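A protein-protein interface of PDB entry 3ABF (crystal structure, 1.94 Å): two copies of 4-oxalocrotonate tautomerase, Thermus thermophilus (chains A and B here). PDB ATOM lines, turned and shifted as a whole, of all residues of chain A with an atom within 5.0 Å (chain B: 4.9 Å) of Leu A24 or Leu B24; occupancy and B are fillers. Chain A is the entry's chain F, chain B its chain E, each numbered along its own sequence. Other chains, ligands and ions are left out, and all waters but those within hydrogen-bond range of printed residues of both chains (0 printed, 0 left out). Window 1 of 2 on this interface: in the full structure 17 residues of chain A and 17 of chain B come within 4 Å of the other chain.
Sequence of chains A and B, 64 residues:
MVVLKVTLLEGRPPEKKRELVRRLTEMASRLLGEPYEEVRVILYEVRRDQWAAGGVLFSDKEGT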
ATOM      1  N   LEU A   4      27.165 -21.166  28.251  1.00  0.00           N
ATOM      2  CA  LEU A   4      26.070 -20.868  27.356  1.00  0.00           C
ATOM      3  C   LEU A   4      25.300 -19.727  27.981  1.00  0.00           C
ATOM      4  O   LEU A   4      24.809 -19.836  29.103  1.00  0.00           O
ATOM      5  CB  LEU A   4      25.161 -22.075  27.199  1.00  0.00           C
ATOM      6  CG  LEU A   4      25.863 -23.329  26.668  1.00  0.00           C
ATOM      7  CD1 LEU A   4      25.269 -24.569  27.324  1.00  0.00           C
ATOM      8  CD2 LEU A   4      25.705 -23.386  25.161  1.00  0.00           C
ATOM      9  N   VAL A   6      22.112 -17.373  27.474  1.00  0.00           N
ATOM     10  CA  VAL A   6      20.885 -17.260  26.720  1.00  0.00           C
ATOM     11  C   VAL A   6      20.310 -15.854  26.928  1.00  0.00           C
ATOM     12  O   VAL A   6      20.080 -15.428  28.070  1.00  0.00           O
ATOM     13  CB  VAL A   6      19.840 -18.264  27.207  1.00  0.00           C
ATOM     14  CG1 VAL A   6      18.651 -18.256  26.243  1.00  0.00           C
ATOM     15  CG2 VAL A   6      20.473 -19.656  27.336  1.00  0.00           C
ATOM     16  N   LEU A  20      14.948 -25.802  30.206  1.00  0.00           N
ATOM     17  CA  LEU A  20      15.877 -25.311  29.188  1.00  0.00           C
ATOM     18  C   LEU A  20      17.315 -25.530  29.641  1.00  0.00           C
ATOM     19  O   LEU A  20      18.143 -26.061  28.897  1.00  0.00           O
ATOM     20  CB  LEU A  20      15.628 -23.822  28.931  1.00  0.00           C
ATOM     21  CG  LEU A  20      16.597 -23.150  27.954  1.00  0.00           C
ATOM     22  CD1 LEU A  20      16.468 -23.797  26.593  1.00  0.00           C
ATOM     23  CD2 LEU A  20      16.305 -21.656  27.884  1.00  0.00           C
ATOM     24  N   VAL A  21      17.610 -25.125  30.870  1.00  0.00           N
ATOM     25  CA  VAL A  21      18.954 -25.281  31.422  1.00  0.00           C
ATOM     26  C   VAL A  21      19.392 -26.747  31.418  1.00  0.00           C
ATOM     27  O   VAL A  21      20.567 -27.069  31.175  1.00  0.00           O
ATOM     28  CB  VAL A  21      19.025 -24.745  32.871  1.00  0.00           C
ATOM     29  CG1 VAL A  21      20.334 -25.168  33.522  1.00  0.00           C
ATOM     30  CG2 VAL A  21      18.909 -23.218  32.870  1.00  0.00           C
ATOM     31  N   ARG A  22      18.443 -27.638  31.683  1.00  0.00           N
ATOM     32  CA  ARG A  22      18.739 -29.060  31.721  1.00  0.00           C
ATOM     33  C   ARG A  22      19.093 -29.600  30.337  1.00  0.00           C
ATOM     34  O   ARG A  22      20.115 -30.267  30.173  1.00  0.00           O
ATOM     35  CB  ARG A  22      17.539 -29.817  32.317  1.00  0.00           C
ATOM     36  CG  ARG A  22      17.655 -31.330  32.279  1.00  0.00           C
ATOM     37  CD  ARG A  22      16.506 -31.973  33.058  1.00  0.00           C
ATOM     38  NE  ARG A  22      15.201 -31.606  32.512  1.00  0.00           N
ATOM     39  CZ  ARG A  22      14.716 -32.058  31.358  1.00  0.00           C
ATOM     40  NH1 ARG A  22      15.427 -32.905  30.621  1.00  0.00           N
ATOM     41  NH2 ARG A  22      13.527 -31.652  30.933  1.00  0.00           N
ATOM     42  N   ARG A  23      18.255 -29.301  29.352  1.00  0.00           N
ATOM     43  CA  ARG A  23      18.469 -29.750  27.977  1.00  0.00           C
ATOM     44  C   ARG A  23      19.747 -29.180  27.358  1.00  0.00           C
ATOM     45  O   ARG A  23      20.470 -29.893  26.665  1.00  0.00           O
ATOM     46  CB  ARG A  23      17.266 -29.373  27.111  1.00  0.00           C
ATOM     47  CG  ARG A  23      15.951 -29.969  27.582  1.00  0.00           C
ATOM     48  CD  ARG A  23      15.957 -31.488  27.522  1.00  0.00           C
ATOM     49  NE  ARG A  23      16.206 -31.989  26.170  1.00  0.00           N
ATOM     50  CZ  ARG A  23      17.380 -32.447  25.741  1.00  0.00           C
ATOM     51  NH1 ARG A  23      18.427 -32.476  26.558  1.00  0.00           N
ATOM     52  NH2 ARG A  23      17.513 -32.876  24.494  1.00  0.00           N
ATOM     53  N   LEU A  24      20.020 -27.898  27.598  1.00  0.00           N
ATOM     54  CA  LEU A  24      21.236 -27.261  27.079  1.00  0.00           C
ATOM     55  C   LEU A  24      22.471 -27.910  27.675  1.00  0.00           C
ATOM     56  O   LEU A  24      23.479 -28.112  26.994  1.00  0.00           O
ATOM     57  CB  LEU A  24      21.287 -25.771  27.437  1.00  0.00           C
ATOM     58  CG  LEU A  24      20.287 -24.796  26.814  1.00  0.00           C
ATOM     59  CD1 LEU A  24      20.462 -23.442  27.488  1.00  0.00           C
ATOM     60  CD2 LEU A  24      20.525 -24.687  25.301  1.00  0.00           C
ATOM     61  N   THR A  25      22.408 -28.227  28.960  1.00  0.00           N
ATOM     62  CA  THR A  25      23.560 -28.826  29.596  1.00  0.00           C
ATOM     63  C   THR A  25      23.829 -30.223  29.052  1.00  0.00           C
ATOM     64  O   THR A  25      24.966 -30.559  28.719  1.00  0.00           O
ATOM     65  CB  THR A  25      23.380 -28.886  31.114  1.00  0.00           C
ATOM     66  OG1 THR A  25      23.141 -27.565  31.607  1.00  0.00           O
ATOM     67  CG2 THR A  25      24.642 -29.436  31.773  1.00  0.00           C
ATOM     68  N   GLU A  26      22.778 -31.026  28.953  1.00  0.00           N
ATOM     69  CA  GLU A  26      22.896 -32.389  28.452  1.00  0.00           C
ATOM     70  C   GLU A  26      23.436 -32.443  27.021  1.00  0.00           C
ATOM     71  O   GLU A  26      24.254 -33.300  26.692  1.00  0.00           O
ATOM     72  CB  GLU A  26      21.534 -33.079  28.538  1.00  0.00           C
ATOM     73  CG  GLU A  26      20.998 -33.149  29.969  1.00  0.00           C
ATOM     74  CD  GLU A  26      19.597 -33.733  30.061  1.00  0.00           C
ATOM     75  OE1 GLU A  26      18.710 -33.299  29.294  1.00  0.00           O
ATOM     76  OE2 GLU A  26      19.380 -34.621  30.912  1.00  0.00           O
ATOM     77  N   MET A  27      22.989 -31.522  26.176  1.00  0.00           N
ATOM     78  CA  MET A  27      23.450 -31.480  24.792  1.00  0.00           C
ATOM     79  C   MET A  27      24.890 -30.995  24.695  1.00  0.00           C
ATOM     80  O   MET A  27      25.709 -31.576  23.985  1.00  0.00           O
ATOM     81  CB  MET A  27      22.562 -30.559  23.969  1.00  0.00           C
ATOM     82  CG  MET A  27      21.211 -31.137  23.621  1.00  0.00           C
ATOM     83  SD  MET A  27      20.160 -29.873  22.886  1.00  0.00           S
ATOM     84  CE  MET A  27      21.347 -28.987  21.862  1.00  0.00           C
ATOM     85  N   ALA A  28      25.190 -29.921  25.410  1.00  0.00           N
ATOM     86  CA  ALA A  28      26.521 -29.355  25.401  1.00  0.00           C
ATOM     87  C   ALA A  28      27.542 -30.346  25.960  1.00  0.00           C
ATOM     88  O   ALA A  28      28.651 -30.480  25.434  1.00  0.00           O
ATOM     89  CB  ALA A  28      26.532 -28.070  26.206  1.00  0.00           C
ATOM     90  N   SER A  29      27.168 -31.030  27.034  1.00  0.00           N
ATOM     91  CA  SER A  29      28.049 -32.005  27.660  1.00  0.00           C
ATOM     92  C   SER A  29      28.365 -33.104  26.657  1.00  0.00           C
ATOM     93  O   SER A  29      29.525 -33.458  26.438  1.00  0.00           O
ATOM     94  CB  SER A  29      27.372 -32.621  28.881  1.00  0.00           C
ATOM     95  OG  SER A  29      28.254 -33.515  29.529  1.00  0.00           O
ATOM     96  N   VAL A  39      29.845 -27.285  32.538  1.00  0.00           N
ATOM     97  CA  VAL A  39      28.873 -26.664  31.647  1.00  0.00           C
ATOM     98  C   VAL A  39      28.076 -25.679  32.488  1.00  0.00           C
ATOM     99  O   VAL A  39      27.346 -26.065  33.402  1.00  0.00           O
ATOM    100  CB  VAL A  39      27.930 -27.701  31.008  1.00  0.00           C
ATOM    101  CG1 VAL A  39      26.893 -26.994  30.141  1.00  0.00           C
ATOM    102  CG2 VAL A  39      28.731 -28.680  30.167  1.00  0.00           C
ATOM    103  N   VAL A  41      25.447 -22.305  32.558  1.00  0.00           N
ATOM    104  CA  VAL A  41      24.442 -21.619  31.769  1.00  0.00           C
ATOM    105  C   VAL A  41      24.077 -20.359  32.541  1.00  0.00           C
ATOM    106  O   VAL A  41      23.924 -20.390  33.769  1.00  0.00           O
ATOM    107  CB  VAL A  41      23.188 -22.491  31.569  1.00  0.00           C
ATOM    108  CG1 VAL A  41      22.137 -21.727  30.758  1.00  0.00           C
ATOM    109  CG2 VAL A  41      23.556 -23.773  30.846  1.00  0.00           C
ATOM    110  N   LEU B   4      21.558 -17.399  21.613  1.00  0.00           N
ATOM    111  CA  LEU B   4      22.336 -18.288  22.444  1.00  0.00           C
ATOM    112  C   LEU B   4      23.792 -18.024  22.090  1.00  0.00           C
ATOM    113  O   LEU B   4      24.197 -18.198  20.939  1.00  0.00           O
ATOM    114  CB  LEU B   4      21.989 -19.740  22.138  1.00  0.00           C
ATOM    115  CG  LEU B   4      20.526 -20.146  22.307  1.00  0.00           C
ATOM    116  CD1 LEU B   4      20.197 -21.295  21.366  1.00  0.00           C
ATOM    117  CD2 LEU B   4      20.278 -20.540  23.750  1.00  0.00           C
ATOM    118  N   VAL B   6      27.622 -19.072  22.771  1.00  0.00           N
ATOM    119  CA  VAL B   6      28.410 -20.151  23.329  1.00  0.00           C
ATOM    120  C   VAL B   6      29.864 -19.697  23.423  1.00  0.00           C
ATOM    121  O   VAL B   6      30.497 -19.399  22.406  1.00  0.00           O
ATOM    122  CB  VAL B   6      28.351 -21.407  22.431  1.00  0.00           C
ATOM    123  CG1 VAL B   6      29.103 -22.543  23.099  1.00  0.00           C
ATOM    124  CG2 VAL B   6      26.887 -21.803  22.159  1.00  0.00           C
ATOM    125  N   GLU B  19      26.809 -29.139  14.233  1.00  0.00           N
ATOM    126  CA  GLU B  19      25.875 -29.988  14.958  1.00  0.00           C
ATOM    127  C   GLU B  19      25.361 -29.271  16.206  1.00  0.00           C
ATOM    128  O   GLU B  19      24.160 -29.297  16.508  1.00  0.00           O
ATOM    129  CB  GLU B  19      26.567 -31.292  15.357  1.00  0.00           C
ATOM    130  CG  GLU B  19      25.609 -32.437  15.634  1.00  0.00           C
ATOM    131  CD  GLU B  19      26.268 -33.611  16.348  1.00  0.00           C
ATOM    132  OE1 GLU B  19      27.351 -34.059  15.909  1.00  0.00           O
ATOM    133  OE2 GLU B  19      25.691 -34.093  17.348  1.00  0.00           O
ATOM    134  N   LEU B  20      26.280 -28.648  16.938  1.00  0.00           N
ATOM    135  CA  LEU B  20      25.914 -27.904  18.140  1.00  0.00           C
ATOM    136  C   LEU B  20      24.882 -26.817  17.798  1.00  0.00           C
ATOM    137  O   LEU B  20      23.851 -26.666  18.467  1.00  0.00           O
ATOM    138  CB  LEU B  20      27.166 -27.263  18.755  1.00  0.00           C
ATOM    139  CG  LEU B  20      26.979 -26.529  20.087  1.00  0.00           C
ATOM    140  CD1 LEU B  20      26.544 -27.516  21.162  1.00  0.00           C
ATOM    141  CD2 LEU B  20      28.273 -25.830  20.477  1.00  0.00           C
ATOM    142  N   VAL B  21      25.159 -26.055  16.750  1.00  0.00           N
ATOM    143  CA  VAL B  21      24.251 -25.000  16.342  1.00  0.00           C
ATOM    144  C   VAL B  21      22.885 -25.552  15.970  1.00  0.00           C
ATOM    145  O   VAL B  21      21.860 -25.015  16.368  1.00  0.00           O
ATOM    146  CB  VAL B  21      24.840 -24.229  15.153  1.00  0.00           C
ATOM    147  CG1 VAL B  21      23.781 -23.369  14.502  1.00  0.00           C
ATOM    148  CG2 VAL B  21      26.012 -23.368  15.651  1.00  0.00           C
ATOM    149  N   ARG B  22      22.879 -26.637  15.204  1.00  0.00           N
ATOM    150  CA  ARG B  22      21.637 -27.255  14.764  1.00  0.00           C
ATOM    151  C   ARG B  22      20.830 -27.770  15.957  1.00  0.00           C
ATOM    152  O   ARG B  22      19.644 -27.472  16.086  1.00  0.00           O
ATOM    153  CB  ARG B  22      21.964 -28.399  13.793  1.00  0.00           C
ATOM    154  CG  ARG B  22      20.782 -28.993  13.058  1.00  0.00           C
ATOM    155  CD  ARG B  22      21.266 -30.024  12.040  1.00  0.00           C
ATOM    156  NE  ARG B  22      21.907 -31.167  12.684  1.00  0.00           N
ATOM    157  CZ  ARG B  22      23.180 -31.518  12.515  1.00  0.00           C
ATOM    158  NH1 ARG B  22      23.970 -30.812  11.712  1.00  0.00           N
ATOM    159  NH2 ARG B  22      23.666 -32.578  13.155  1.00  0.00           N
ATOM    160  N   ARG B  23      21.479 -28.532  16.831  1.00  0.00           N
ATOM    161  CA  ARG B  23      20.818 -29.088  18.017  1.00  0.00           C
ATOM    162  C   ARG B  23      20.302 -28.005  18.980  1.00  0.00           C
ATOM    163  O   ARG B  23      19.183 -28.096  19.500  1.00  0.00           O
ATOM    164  CB  ARG B  23      21.786 -30.005  18.767  1.00  0.00           C
ATOM    165  CG  ARG B  23      22.234 -31.231  17.994  1.00  0.00           C
ATOM    166  CD  ARG B  23      21.116 -32.249  17.856  1.00  0.00           C
ATOM    167  NE  ARG B  23      21.606 -33.615  18.045  1.00  0.00           N
ATOM    168  CZ  ARG B  23      22.457 -34.233  17.229  1.00  0.00           C
ATOM    169  NH1 ARG B  23      22.925 -33.614  16.152  1.00  0.00           N
ATOM    170  NH2 ARG B  23      22.845 -35.473  17.495  1.00  0.00           N
ATOM    171  N   LEU B  24      21.123 -26.992  19.237  1.00  0.00           N
ATOM    172  CA  LEU B  24      20.729 -25.905  20.132  1.00  0.00           C
ATOM    173  C   LEU B  24      19.481 -25.201  19.600  1.00  0.00           C
ATOM    174  O   LEU B  24      18.555 -24.900  20.360  1.00  0.00           O
ATOM    175  CB  LEU B  24      21.852 -24.869  20.261  1.00  0.00           C
ATOM    176  CG  LEU B  24      23.189 -25.214  20.928  1.00  0.00           C
ATOM    177  CD1 LEU B  24      24.131 -24.017  20.789  1.00  0.00           C
ATOM    178  CD2 LEU B  24      22.974 -25.559  22.395  1.00  0.00           C
ATOM    179  N   THR B  25      19.460 -24.959  18.289  1.00  0.00           N
ATOM    180  CA  THR B  25      18.354 -24.278  17.648  1.00  0.00           C
ATOM    181  C   THR B  25      17.052 -25.071  17.716  1.00  0.00           C
ATOM    182  O   THR B  25      16.015 -24.525  18.058  1.00  0.00           O
ATOM    183  CB  THR B  25      18.696 -23.957  16.186  1.00  0.00           C
ATOM    184  OG1 THR B  25      19.955 -23.273  16.132  1.00  0.00           O
ATOM    185  CG2 THR B  25      17.633 -23.045  15.570  1.00  0.00           C
ATOM    186  N   GLU B  26      17.112 -26.359  17.401  1.00  0.00           N
ATOM    187  CA  GLU B  26      15.919 -27.209  17.440  1.00  0.00           C
ATOM    188  C   GLU B  26      15.312 -27.204  18.835  1.00  0.00           C
ATOM    189  O   GLU B  26      14.121 -26.967  19.022  1.00  0.00           O
ATOM    190  CB  GLU B  26      16.283 -28.641  17.040  1.00  0.00           C
ATOM    191  N   MET B  27      16.162 -27.445  19.817  1.00  0.00           N
ATOM    192  CA  MET B  27      15.743 -27.498  21.199  1.00  0.00           C
ATOM    193  C   MET B  27      15.232 -26.158  21.743  1.00  0.00           C
ATOM    194  O   MET B  27      14.212 -26.113  22.436  1.00  0.00           O
ATOM    195  CB  MET B  27      16.901 -28.043  22.033  1.00  0.00           C
ATOM    196  CG  MET B  27      16.528 -28.413  23.434  1.00  0.00           C
ATOM    197  SD  MET B  27      16.484 -26.953  24.445  1.00  0.00           S
ATOM    198  CE  MET B  27      18.259 -26.680  24.651  1.00  0.00           C
ATOM    199  N   ALA B  28      15.919 -25.066  21.438  1.00  0.00           N
ATOM    200  CA  ALA B  28      15.463 -23.764  21.919  1.00  0.00           C
ATOM    201  C   ALA B  28      14.142 -23.404  21.243  1.00  0.00           C
ATOM    202  O   ALA B  28      13.229 -22.859  21.871  1.00  0.00           O
ATOM    203  CB  ALA B  28      16.512 -22.697  21.627  1.00  0.00           C
ATOM    204  N   SER B  29      14.038 -23.725  19.958  1.00  0.00           N
ATOM    205  CA  SER B  29      12.838 -23.418  19.196  1.00  0.00           C
ATOM    206  C   SER B  29      11.602 -24.119  19.741  1.00  0.00           C
ATOM    207  O   SER B  29      10.579 -23.483  20.008  1.00  0.00           O
ATOM    208  CB  SER B  29      13.023 -23.822  17.739  1.00  0.00           C
ATOM    209  OG  SER B  29      11.846 -23.522  17.022  1.00  0.00           O
ATOM    210  N   VAL B  41      22.353 -18.200  17.075  1.00  0.00           N
ATOM    211  CA  VAL B  41      23.473 -18.704  17.850  1.00  0.00           C
ATOM    212  C   VAL B  41      24.743 -17.961  17.434  1.00  0.00           C
ATOM    213  O   VAL B  41      25.005 -17.770  16.240  1.00  0.00           O
ATOM    214  CB  VAL B  41      23.710 -20.214  17.612  1.00  0.00           C
ATOM    215  CG1 VAL B  41      24.882 -20.701  18.454  1.00  0.00           C
ATOM    216  CG2 VAL B  41      22.457 -21.015  17.942  1.00  0.00           C
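The guanidinium group (NH1) of Arg A23 lies within salt-bridge range of the side-chain carboxylate (OE1) of Glu A26, 2.9 Å away.
The guanidinium group (NH1) of Arg B23 lies within salt-bridge range of the side-chain carboxylate (OE2) of Glu B19.
Among the printed residues, merely in contact across the chains: Leu A24 with Met B27 (3.1 Å), Met A27 with Arg B23 (3.2 Å), Met A27 with Leu B24 (3.3 Å), Leu A4 with Val B6 (3.6 Å), Arg A23 with Met B27 (3.7 Å), Val A6 with Leu B4 (3.7 Å), Leu A20 with Met B27 (3.8 Å), Met A27 with Met B27 (3.8 Å) and Leu A24 with Leu B24 (3.9 Å).
Leu A24 touches just these residues of chain B: Leu B24 (3.9 Å) and Met B27 (3.1 Å).
Printed residues of chain A within 4 Å of Leu B24: Leu A24 (3.9 Å) and Met A27 (3.3 Å).
Of the printed residues of chain B, Leu A4 touches Val B6.
Of the printed residues of chain A, Arg B23 touches Met A27 (3.2 Å).
Of the printed residues of chain A, Val B6 touches Leu A4.
Of the printed residues of chain B, Val A6 touches Leu B4 (3.7 Å).
Ser A29 touches none of the printed residues of chain B.
The nearest residue of chain B that does not touch Leu A24 is Leu B4 (4.4 Å).
The nearest residue of chain A that does not touch Leu B24 is Leu A4 (4.5 Å).
Printed residues of chain B that touch a printed residue of chain A: Leu B4, Val B6, Arg B23, Leu B24 and Met B27.
Hydrophobic or aromatic side chains of chain B within 4 Å of the printed part of chain A: Leu B4, Val B6, Leu B24 and Met B27.
Of the 14 printed residues of chain A, 6 touch a printed residue of chain B.
Hydrophobic or aromatic side chains of chain A that line the printed part of chain B: Leu A4, Val A6, Leu A20, Leu A24 and Met A27.
Along chain A the printed residues that touch a printed residue of chain B span positions 4 to 27.
Among the printed residues, 9 pairs touch across the chains.
Among the printed residues, no Asp or Glu carboxylate lies within 4 Å of a Lys or Arg side-chain nitrogen of the other chain.
Leu A20 touches Met B27, but with the chains exchanged Met A27 does not touch Leu B20 (4.8 Å).
Arg A23 touches Met B27, and with the chains exchanged Met A27 touches Arg B23.
Leu B24 touches its own counterpart, Leu A24.
Leu A24 touches Met B27, and with the chains exchanged Met A27 touches Leu B24.
Of the 9 pairs that touch across the chains among the printed residues, 8 have their exchanged pair printed and touching as well.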
